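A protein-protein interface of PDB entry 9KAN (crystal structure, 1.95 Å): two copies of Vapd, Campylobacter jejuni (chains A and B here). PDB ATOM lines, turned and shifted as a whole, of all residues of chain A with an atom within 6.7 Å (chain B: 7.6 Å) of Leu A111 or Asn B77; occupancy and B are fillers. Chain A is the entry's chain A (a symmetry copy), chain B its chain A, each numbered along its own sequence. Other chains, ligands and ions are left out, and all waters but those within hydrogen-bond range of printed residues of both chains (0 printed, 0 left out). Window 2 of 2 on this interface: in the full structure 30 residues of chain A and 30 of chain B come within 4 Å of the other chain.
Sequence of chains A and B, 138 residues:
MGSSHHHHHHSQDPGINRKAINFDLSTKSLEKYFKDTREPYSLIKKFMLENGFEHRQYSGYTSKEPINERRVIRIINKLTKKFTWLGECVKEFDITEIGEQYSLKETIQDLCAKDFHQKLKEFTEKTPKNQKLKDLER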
ATOM      1  N   GLU A 106       3.505  11.086  19.319  1.00  0.00           N
ATOM      2  CA  GLU A 106       3.514   9.884  18.497  1.00  0.00           C
ATOM      3  C   GLU A 106       2.108   9.316  18.288  1.00  0.00           C
ATOM      4  O   GLU A 106       1.816   8.776  17.215  1.00  0.00           O
ATOM      5  CB  GLU A 106       4.436   8.844  19.135  1.00  0.00           C
ATOM      6  CG  GLU A 106       4.208   7.416  18.670  1.00  0.00           C
ATOM      7  CD  GLU A 106       4.816   7.131  17.304  1.00  0.00           C
ATOM      8  OE1 GLU A 106       4.138   7.343  16.276  1.00  0.00           O
ATOM      9  OE2 GLU A 106       5.981   6.683  17.255  1.00  0.00           O
ATOM     10  N   THR A 107       1.228   9.420  19.291  1.00  0.00           N
ATOM     11  CA  THR A 107      -0.131   8.911  19.134  1.00  0.00           C
ATOM     12  C   THR A 107      -0.872   9.660  18.037  1.00  0.00           C
ATOM     13  O   THR A 107      -1.566   9.049  17.217  1.00  0.00           O
ATOM     14  CB  THR A 107      -0.895   9.028  20.447  1.00  0.00           C
ATOM     15  OG1 THR A 107      -0.078   8.544  21.518  1.00  0.00           O
ATOM     16  CG2 THR A 107      -2.177   8.195  20.386  1.00  0.00           C
ATOM     17  N   ILE A 108      -0.739  10.986  18.022  1.00  0.00           N
ATOM     18  CA  ILE A 108      -1.352  11.825  16.993  1.00  0.00           C
ATOM     19  C   ILE A 108      -0.792  11.481  15.614  1.00  0.00           C
ATOM     20  O   ILE A 108      -1.536  11.398  14.626  1.00  0.00           O
ATOM     21  CB  ILE A 108      -1.140  13.310  17.367  1.00  0.00           C
ATOM     22  CG1 ILE A 108      -2.094  13.703  18.512  1.00  0.00           C
ATOM     23  CG2 ILE A 108      -1.261  14.228  16.150  1.00  0.00           C
ATOM     24  CD1 ILE A 108      -1.784  15.032  19.159  1.00  0.00           C
ATOM     25  N   GLN A 109       0.523  11.253  15.525  1.00  0.00           N
ATOM     26  CA  GLN A 109       1.109  10.756  14.281  1.00  0.00           C
ATOM     27  C   GLN A 109       0.520   9.396  13.888  1.00  0.00           C
ATOM     28  O   GLN A 109       0.231   9.154  12.707  1.00  0.00           O
ATOM     29  CB  GLN A 109       2.636  10.689  14.421  1.00  0.00           C
ATOM     30  CG  GLN A 109       3.308  12.072  14.599  1.00  0.00           C
ATOM     31  CD  GLN A 109       4.773  11.979  15.041  1.00  0.00           C
ATOM     32  OE1 GLN A 109       5.212  10.938  15.526  1.00  0.00           O
ATOM     33  NE2 GLN A 109       5.527  13.067  14.874  1.00  0.00           N
ATOM     34  N   ASP A 110       0.307   8.505  14.869  1.00  0.00           N
ATOM     35  CA  ASP A 110      -0.283   7.194  14.593  1.00  0.00           C
ATOM     36  C   ASP A 110      -1.700   7.323  14.061  1.00  0.00           C
ATOM     37  O   ASP A 110      -2.069   6.641  13.099  1.00  0.00           O
ATOM     38  CB  ASP A 110      -0.298   6.328  15.856  1.00  0.00           C
ATOM     39  CG  ASP A 110       0.998   5.569  16.062  1.00  0.00           C
ATOM     40  OD1 ASP A 110       1.979   5.868  15.352  1.00  0.00           O
ATOM     41  OD2 ASP A 110       1.030   4.666  16.932  1.00  0.00           O
ATOM     42  N   LEU A 111      -2.514   8.170  14.692  1.00  0.00           N
ATOM     43  CA  LEU A 111      -3.908   8.298  14.284  1.00  0.00           C
ATOM     44  C   LEU A 111      -4.017   8.736  12.829  1.00  0.00           C
ATOM     45  O   LEU A 111      -4.836   8.200  12.072  1.00  0.00           O
ATOM     46  CB  LEU A 111      -4.632   9.280  15.206  1.00  0.00           C
ATOM     47  CG  LEU A 111      -4.917   8.797  16.631  1.00  0.00           C
ATOM     48  CD1 LEU A 111      -5.281   9.977  17.531  1.00  0.00           C
ATOM     49  CD2 LEU A 111      -6.006   7.716  16.667  1.00  0.00           C
ATOM     50  N   CYS A 112      -3.155   9.655  12.414  1.00  0.00           N
ATOM     51  CA  CYS A 112      -3.201  10.171  11.024  1.00  0.00           C
ATOM     52  C   CYS A 112      -2.374   9.253  10.102  1.00  0.00           C
ATOM     53  O   CYS A 112      -1.668   9.795   9.242  1.00  0.00           O
ATOM     54  CB  CYS A 112      -2.675  11.603  10.991  1.00  0.00           C
ATOM     55  SG  CYS A 112      -3.327  12.699  12.276  1.00  0.00           S
ATOM     56  N   ALA A 113      -2.487   7.930  10.266  1.00  0.00           N
ATOM     57  CA  ALA A 113      -1.748   6.978   9.399  1.00  0.00           C
ATOM     58  C   ALA A 113      -2.713   6.241   8.466  1.00  0.00           C
ATOM     59  O   ALA A 113      -2.235   5.640   7.482  1.00  0.00           O
ATOM     60  CB  ALA A 113      -0.949   6.006  10.240  1.00  0.00           C
ATOM     61  N   LYS A 114      -4.008   6.281   8.750  1.00  0.00           N
ATOM     62  CA  LYS A 114      -4.954   5.650   7.799  1.00  0.00           C
ATOM     63  C   LYS A 114      -4.310   4.361   7.274  1.00  0.00           C
ATOM     64  O   LYS A 114      -4.097   4.254   6.045  1.00  0.00           O
ATOM     65  CB  LYS A 114      -5.299   6.624   6.668  1.00  0.00           C
ATOM     66  CG  LYS A 114      -4.103   7.036   5.827  1.00  0.00           C
ATOM     67  CD  LYS A 114      -4.483   8.004   4.713  1.00  0.00           C
ATOM     68  CE  LYS A 114      -4.901   9.328   5.263  1.00  0.00           C
ATOM     69  NZ  LYS A 114      -5.267  10.261   4.196  1.00  0.00           N
ATOM     70  N   ASP A 115      -4.003   3.432   8.177  1.00  0.00           N
ATOM     71  CA  ASP A 115      -3.454   2.120   7.734  1.00  0.00           C
ATOM     72  C   ASP A 115      -4.466   1.061   8.152  1.00  0.00           C
ATOM     73  O   ASP A 115      -4.418  -0.058   7.612  1.00  0.00           O
ATOM     74  CB  ASP A 115      -2.111   1.823   8.370  1.00  0.00           C
ATOM     75  CG  ASP A 115      -1.971   2.235   9.830  1.00  0.00           C
ATOM     76  OD1 ASP A 115      -2.974   2.693  10.414  1.00  0.00           O
ATOM     77  OD2 ASP A 115      -0.859   2.089  10.372  1.00  0.00           O
ATOM     78  N   PHE B  47     -11.857  25.225  17.843  1.00  0.00           N
ATOM     79  CA  PHE B  47     -12.244  23.867  18.218  1.00  0.00           C
ATOM     80  C   PHE B  47     -12.120  23.651  19.719  1.00  0.00           C
ATOM     81  O   PHE B  47     -12.953  22.975  20.339  1.00  0.00           O
ATOM     82  CB  PHE B  47     -11.369  22.861  17.471  1.00  0.00           C
ATOM     83  CG  PHE B  47     -11.583  21.427  17.891  1.00  0.00           C
ATOM     84  CD1 PHE B  47     -10.925  20.890  19.004  1.00  0.00           C
ATOM     85  CD2 PHE B  47     -12.430  20.606  17.164  1.00  0.00           C
ATOM     86  CE1 PHE B  47     -11.121  19.580  19.382  1.00  0.00           C
ATOM     87  CE2 PHE B  47     -12.631  19.290  17.540  1.00  0.00           C
ATOM     88  CZ  PHE B  47     -11.975  18.777  18.645  1.00  0.00           C
ATOM     89  N   ARG B  71     -12.598  11.283  28.279  1.00  0.00           N
ATOM     90  CA  ARG B  71     -13.216  12.341  27.483  1.00  0.00           C
ATOM     91  C   ARG B  71     -12.178  13.237  26.820  1.00  0.00           C
ATOM     92  O   ARG B  71     -12.400  13.718  25.700  1.00  0.00           O
ATOM     93  CB  ARG B  71     -14.165  13.156  28.361  1.00  0.00           C
ATOM     94  CG  ARG B  71     -15.450  12.382  28.749  1.00  0.00           C
ATOM     95  CD  ARG B  71     -16.385  13.223  29.620  1.00  0.00           C
ATOM     96  NE  ARG B  71     -15.836  13.351  30.965  1.00  0.00           N
ATOM     97  CZ  ARG B  71     -15.965  14.420  31.744  1.00  0.00           C
ATOM     98  NH1 ARG B  71     -16.636  15.493  31.347  1.00  0.00           N
ATOM     99  NH2 ARG B  71     -15.401  14.413  32.949  1.00  0.00           N
ATOM    100  N   VAL B  72     -11.042  13.459  27.484  1.00  0.00           N
ATOM    101  CA  VAL B  72      -9.961  14.257  26.906  1.00  0.00           C
ATOM    102  C   VAL B  72      -9.423  13.595  25.650  1.00  0.00           C
ATOM    103  O   VAL B  72      -9.251  14.234  24.606  1.00  0.00           O
ATOM    104  CB  VAL B  72      -8.834  14.472  27.938  1.00  0.00           C
ATOM    105  CG1 VAL B  72      -7.593  15.030  27.260  1.00  0.00           C
ATOM    106  CG2 VAL B  72      -9.310  15.404  29.022  1.00  0.00           C
ATOM    107  N   ILE B  73      -9.141  12.298  25.727  1.00  0.00           N
ATOM    108  CA  ILE B  73      -8.566  11.667  24.551  1.00  0.00           C
ATOM    109  C   ILE B  73      -9.605  11.525  23.431  1.00  0.00           C
ATOM    110  O   ILE B  73      -9.232  11.440  22.255  1.00  0.00           O
ATOM    111  CB  ILE B  73      -7.925  10.316  24.904  1.00  0.00           C
ATOM    112  CG1 ILE B  73      -8.992   9.332  25.271  1.00  0.00           C
ATOM    113  CG2 ILE B  73      -6.835  10.431  26.002  1.00  0.00           C
ATOM    114  CD1 ILE B  73      -9.096   8.296  24.212  1.00  0.00           C
ATOM    115  N   ARG B  74     -10.906  11.462  23.760  1.00  0.00           N
ATOM    116  CA  ARG B  74     -11.916  11.504  22.696  1.00  0.00           C
ATOM    117  C   ARG B  74     -11.910  12.853  21.980  1.00  0.00           C
ATOM    118  O   ARG B  74     -12.083  12.912  20.759  1.00  0.00           O
ATOM    119  CB  ARG B  74     -13.316  11.210  23.232  1.00  0.00           C
ATOM    120  CG  ARG B  74     -13.569   9.741  23.575  1.00  0.00           C
ATOM    121  CD  ARG B  74     -15.070   9.379  23.611  1.00  0.00           C
ATOM    122  NE  ARG B  74     -15.738   9.522  22.313  1.00  0.00           N
ATOM    123  CZ  ARG B  74     -16.684  10.416  22.034  1.00  0.00           C
ATOM    124  NH1 ARG B  74     -17.098  11.299  22.928  1.00  0.00           N
ATOM    125  NH2 ARG B  74     -17.221  10.431  20.814  1.00  0.00           N
ATOM    126  N   ILE B  75     -11.690  13.936  22.721  1.00  0.00           N
ATOM    127  CA  ILE B  75     -11.588  15.261  22.123  1.00  0.00           C
ATOM    128  C   ILE B  75     -10.355  15.352  21.230  1.00  0.00           C
ATOM    129  O   ILE B  75     -10.401  15.943  20.146  1.00  0.00           O
ATOM    130  CB  ILE B  75     -11.594  16.325  23.241  1.00  0.00           C
ATOM    131  CG1 ILE B  75     -13.011  16.460  23.808  1.00  0.00           C
ATOM    132  CG2 ILE B  75     -11.005  17.645  22.777  1.00  0.00           C
ATOM    133  CD1 ILE B  75     -13.070  17.098  25.187  1.00  0.00           C
ATOM    134  N   ILE B  76      -9.245  14.741  21.646  1.00  0.00           N
ATOM    135  CA  ILE B  76      -8.033  14.789  20.831  1.00  0.00           C
ATOM    136  C   ILE B  76      -8.190  13.926  19.580  1.00  0.00           C
ATOM    137  O   ILE B  76      -7.723  14.292  18.491  1.00  0.00           O
ATOM    138  CB  ILE B  76      -6.807  14.363  21.658  1.00  0.00           C
ATOM    139  CG1 ILE B  76      -6.631  15.269  22.888  1.00  0.00           C
ATOM    140  CG2 ILE B  76      -5.553  14.401  20.787  1.00  0.00           C
ATOM    141  CD1 ILE B  76      -6.426  16.749  22.549  1.00  0.00           C
ATOM    142  N   ASN B  77      -8.824  12.762  19.720  1.00  0.00           N
ATOM    143  CA  ASN B  77      -9.199  11.954  18.554  1.00  0.00           C
ATOM    144  C   ASN B  77     -10.044  12.764  17.580  1.00  0.00           C
ATOM    145  O   ASN B  77      -9.742  12.837  16.381  1.00  0.00           O
ATOM    146  CB  ASN B  77      -9.957  10.710  19.023  1.00  0.00           C
ATOM    147  CG  ASN B  77     -10.045   9.620  17.957  1.00  0.00           C
ATOM    148  OD1 ASN B  77     -11.067   8.952  17.831  1.00  0.00           O
ATOM    149  ND2 ASN B  77      -8.967   9.421  17.212  1.00  0.00           N
ATOM    150  N   LYS B  78     -11.110  13.384  18.089  1.00  0.00           N
ATOM    151  CA  LYS B  78     -11.959  14.258  17.285  1.00  0.00           C
ATOM    152  C   LYS B  78     -11.145  15.349  16.585  1.00  0.00           C
ATOM    153  O   LYS B  78     -11.333  15.607  15.385  1.00  0.00           O
ATOM    154  CB  LYS B  78     -13.029  14.864  18.194  1.00  0.00           C
ATOM    155  CG  LYS B  78     -14.008  15.808  17.552  1.00  0.00           C
ATOM    156  CD  LYS B  78     -14.867  16.446  18.635  1.00  0.00           C
ATOM    157  CE  LYS B  78     -16.227  16.849  18.110  1.00  0.00           C
ATOM    158  NZ  LYS B  78     -17.097  17.258  19.251  1.00  0.00           N
ATOM    159  N   LEU B  79     -10.231  15.999  17.323  1.00  0.00           N
ATOM    160  CA  LEU B  79      -9.378  17.035  16.739  1.00  0.00           C
ATOM    161  C   LEU B  79      -8.516  16.493  15.602  1.00  0.00           C
ATOM    162  O   LEU B  79      -8.389  17.139  14.549  1.00  0.00           O
ATOM    163  CB  LEU B  79      -8.496  17.652  17.819  1.00  0.00           C
ATOM    164  CG  LEU B  79      -7.454  18.694  17.420  1.00  0.00           C
ATOM    165  CD1 LEU B  79      -8.103  20.018  17.014  1.00  0.00           C
ATOM    166  CD2 LEU B  79      -6.421  18.881  18.563  1.00  0.00           C
ATOM    167  N   THR B  80      -7.889  15.325  15.796  1.00  0.00           N
ATOM    168  CA  THR B  80      -6.991  14.813  14.762  1.00  0.00           C
ATOM    169  C   THR B  80      -7.756  14.338  13.535  1.00  0.00           C
ATOM    170  O   THR B  80      -7.225  14.412  12.426  1.00  0.00           O
ATOM    171  CB  THR B  80      -6.130  13.663  15.281  1.00  0.00           C
ATOM    172  OG1 THR B  80      -6.961  12.515  15.500  1.00  0.00           O
ATOM    173  CG2 THR B  80      -5.396  14.059  16.563  1.00  0.00           C
ATOM    174  N   LYS B  81      -8.990  13.837  13.708  1.00  0.00           N
ATOM    175  CA  LYS B  81      -9.805  13.499  12.541  1.00  0.00           C
ATOM    176  C   LYS B  81     -10.258  14.753  11.796  1.00  0.00           C
ATOM    177  O   LYS B  81     -10.375  14.739  10.565  1.00  0.00           O
ATOM    178  CB  LYS B  81     -11.002  12.645  12.956  1.00  0.00           C
ATOM    179  CG  LYS B  81     -10.594  11.235  13.351  1.00  0.00           C
ATOM    180  CD  LYS B  81     -11.725  10.451  13.952  1.00  0.00           C
ATOM    181  CE  LYS B  81     -11.341   8.976  14.062  1.00  0.00           C
ATOM    182  NZ  LYS B  81     -11.751   8.408  15.375  1.00  0.00           N
ATOM    183  N   LYS B  82     -10.479  15.852  12.514  1.00  0.00           N
ATOM    184  CA  LYS B  82     -10.879  17.088  11.857  1.00  0.00           C
ATOM    185  C   LYS B  82      -9.716  17.718  11.091  1.00  0.00           C
ATOM    186  O   LYS B  82      -9.879  18.128   9.938  1.00  0.00           O
ATOM    187  CB  LYS B  82     -11.460  18.056  12.889  1.00  0.00           C
ATOM    188  CG  LYS B  82     -12.074  19.315  12.289  1.00  0.00           C
ATOM    189  CD  LYS B  82     -12.763  20.169  13.345  1.00  0.00           C
ATOM    190  CE  LYS B  82     -13.358  21.427  12.735  1.00  0.00           C
ATOM    191  NZ  LYS B  82     -14.572  21.115  11.935  1.00  0.00           N
ATOM    192  N   PHE B  83      -8.530  17.785  11.690  1.00  0.00           N
ATOM    193  CA  PHE B  83      -7.389  18.462  11.065  1.00  0.00           C
ATOM    194  C   PHE B  83      -6.265  17.459  10.854  1.00  0.00           C
ATOM    195  O   PHE B  83      -5.322  17.411  11.642  1.00  0.00           O
ATOM    196  CB  PHE B  83      -6.913  19.661  11.922  1.00  0.00           C
ATOM    197  CG  PHE B  83      -7.954  20.727  12.095  1.00  0.00           C
ATOM    198  CD1 PHE B  83      -8.403  21.450  11.007  1.00  0.00           C
ATOM    199  CD2 PHE B  83      -8.492  21.006  13.341  1.00  0.00           C
ATOM    200  CE1 PHE B  83      -9.378  22.440  11.157  1.00  0.00           C
ATOM    201  CE2 PHE B  83      -9.462  21.995  13.494  1.00  0.00           C
ATOM    202  CZ  PHE B  83      -9.895  22.714  12.403  1.00  0.00           C
ATOM    203  N   THR B  84      -6.348  16.671   9.778  1.00  0.00           N
ATOM    204  CA  THR B  84      -5.370  15.592   9.616  1.00  0.00           C
ATOM    205  C   THR B  84      -3.952  16.097   9.368  1.00  0.00           C
ATOM    206  O   THR B  84      -3.013  15.298   9.441  1.00  0.00           O
ATOM    207  CB  THR B  84      -5.780  14.661   8.482  1.00  0.00           C
ATOM    208  OG1 THR B  84      -6.105  15.447   7.334  1.00  0.00           O
ATOM    209  CG2 THR B  84      -6.983  13.843   8.871  1.00  0.00           C
ATOM    210  N   GLY B  87      -0.903  15.624  12.325  1.00  0.00           N
ATOM    211  CA  GLY B  87       0.108  14.581  12.431  1.00  0.00           C
ATOM    212  C   GLY B  87       1.397  14.953  11.724  1.00  0.00           C
ATOM    213  O   GLY B  87       2.491  14.640  12.199  1.00  0.00           O
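Among the printed residues, merely in contact across the chains: Leu A111 with Asn B77, Gln A109 with Gly B87, Leu A111 with Thr B80, Ile A108 with Thr B80, Cys A112 with Thr B84 and Ile A108 with Gly B87.
Printed residues of chain B within 4 Å of Leu A111: Asn B77 and Thr B80.
Printed residues of chain B within 4 Å of Cys A112: Thr B84 (3.9 Å) and Gly B87 (3.8 Å).
Asn B77 touches just one residue of chain A: Leu A111 (3.5 Å).
Of the printed residues of chain A, Thr B80 touches Ile A108 and Leu A111.
Printed residues of chain A within 4 Å of Gly B87: Ile A108, Gln A109 and Cys A112.
No position is printed for both chains.
Of the 7 pairs that touch across the chains among the printed residues, none has its exchanged pair printed and touching as well.
The backbone NH (N) of Gly B87 sits at hydrogen-bond distance from the side-chain sulfur (SG) of Cys A112, at 3.8 Å.
Of the 10 printed residues of chain A, 4 touch a printed residue of chain B.
Hydrophobic or aromatic side chains of chain A within 4 Å of the printed part of chain B: Ile A108 and Leu A111.
Among the printed residues, 7 pairs touch across the chains.
Among the printed residues, no Asp or Glu carboxylate lies within 4 Å of a Lys or Arg side-chain nitrogen of the other chain.
The side-chain sulfur (SG) of Cys A112 lies within hydrogen-bond range of the backbone carbonyl oxygen (O) of Ile A108, 3.2 Å away.
The backbone carbonyl oxygen of Asn B77 is in hydrogen-bond range of the side-chain hydroxyl of Thr B80 (2.9 Å).
NZ of Lys B81 sits at hydrogen-bond distance from OD1 of Asn B77, 2.6 Å away.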
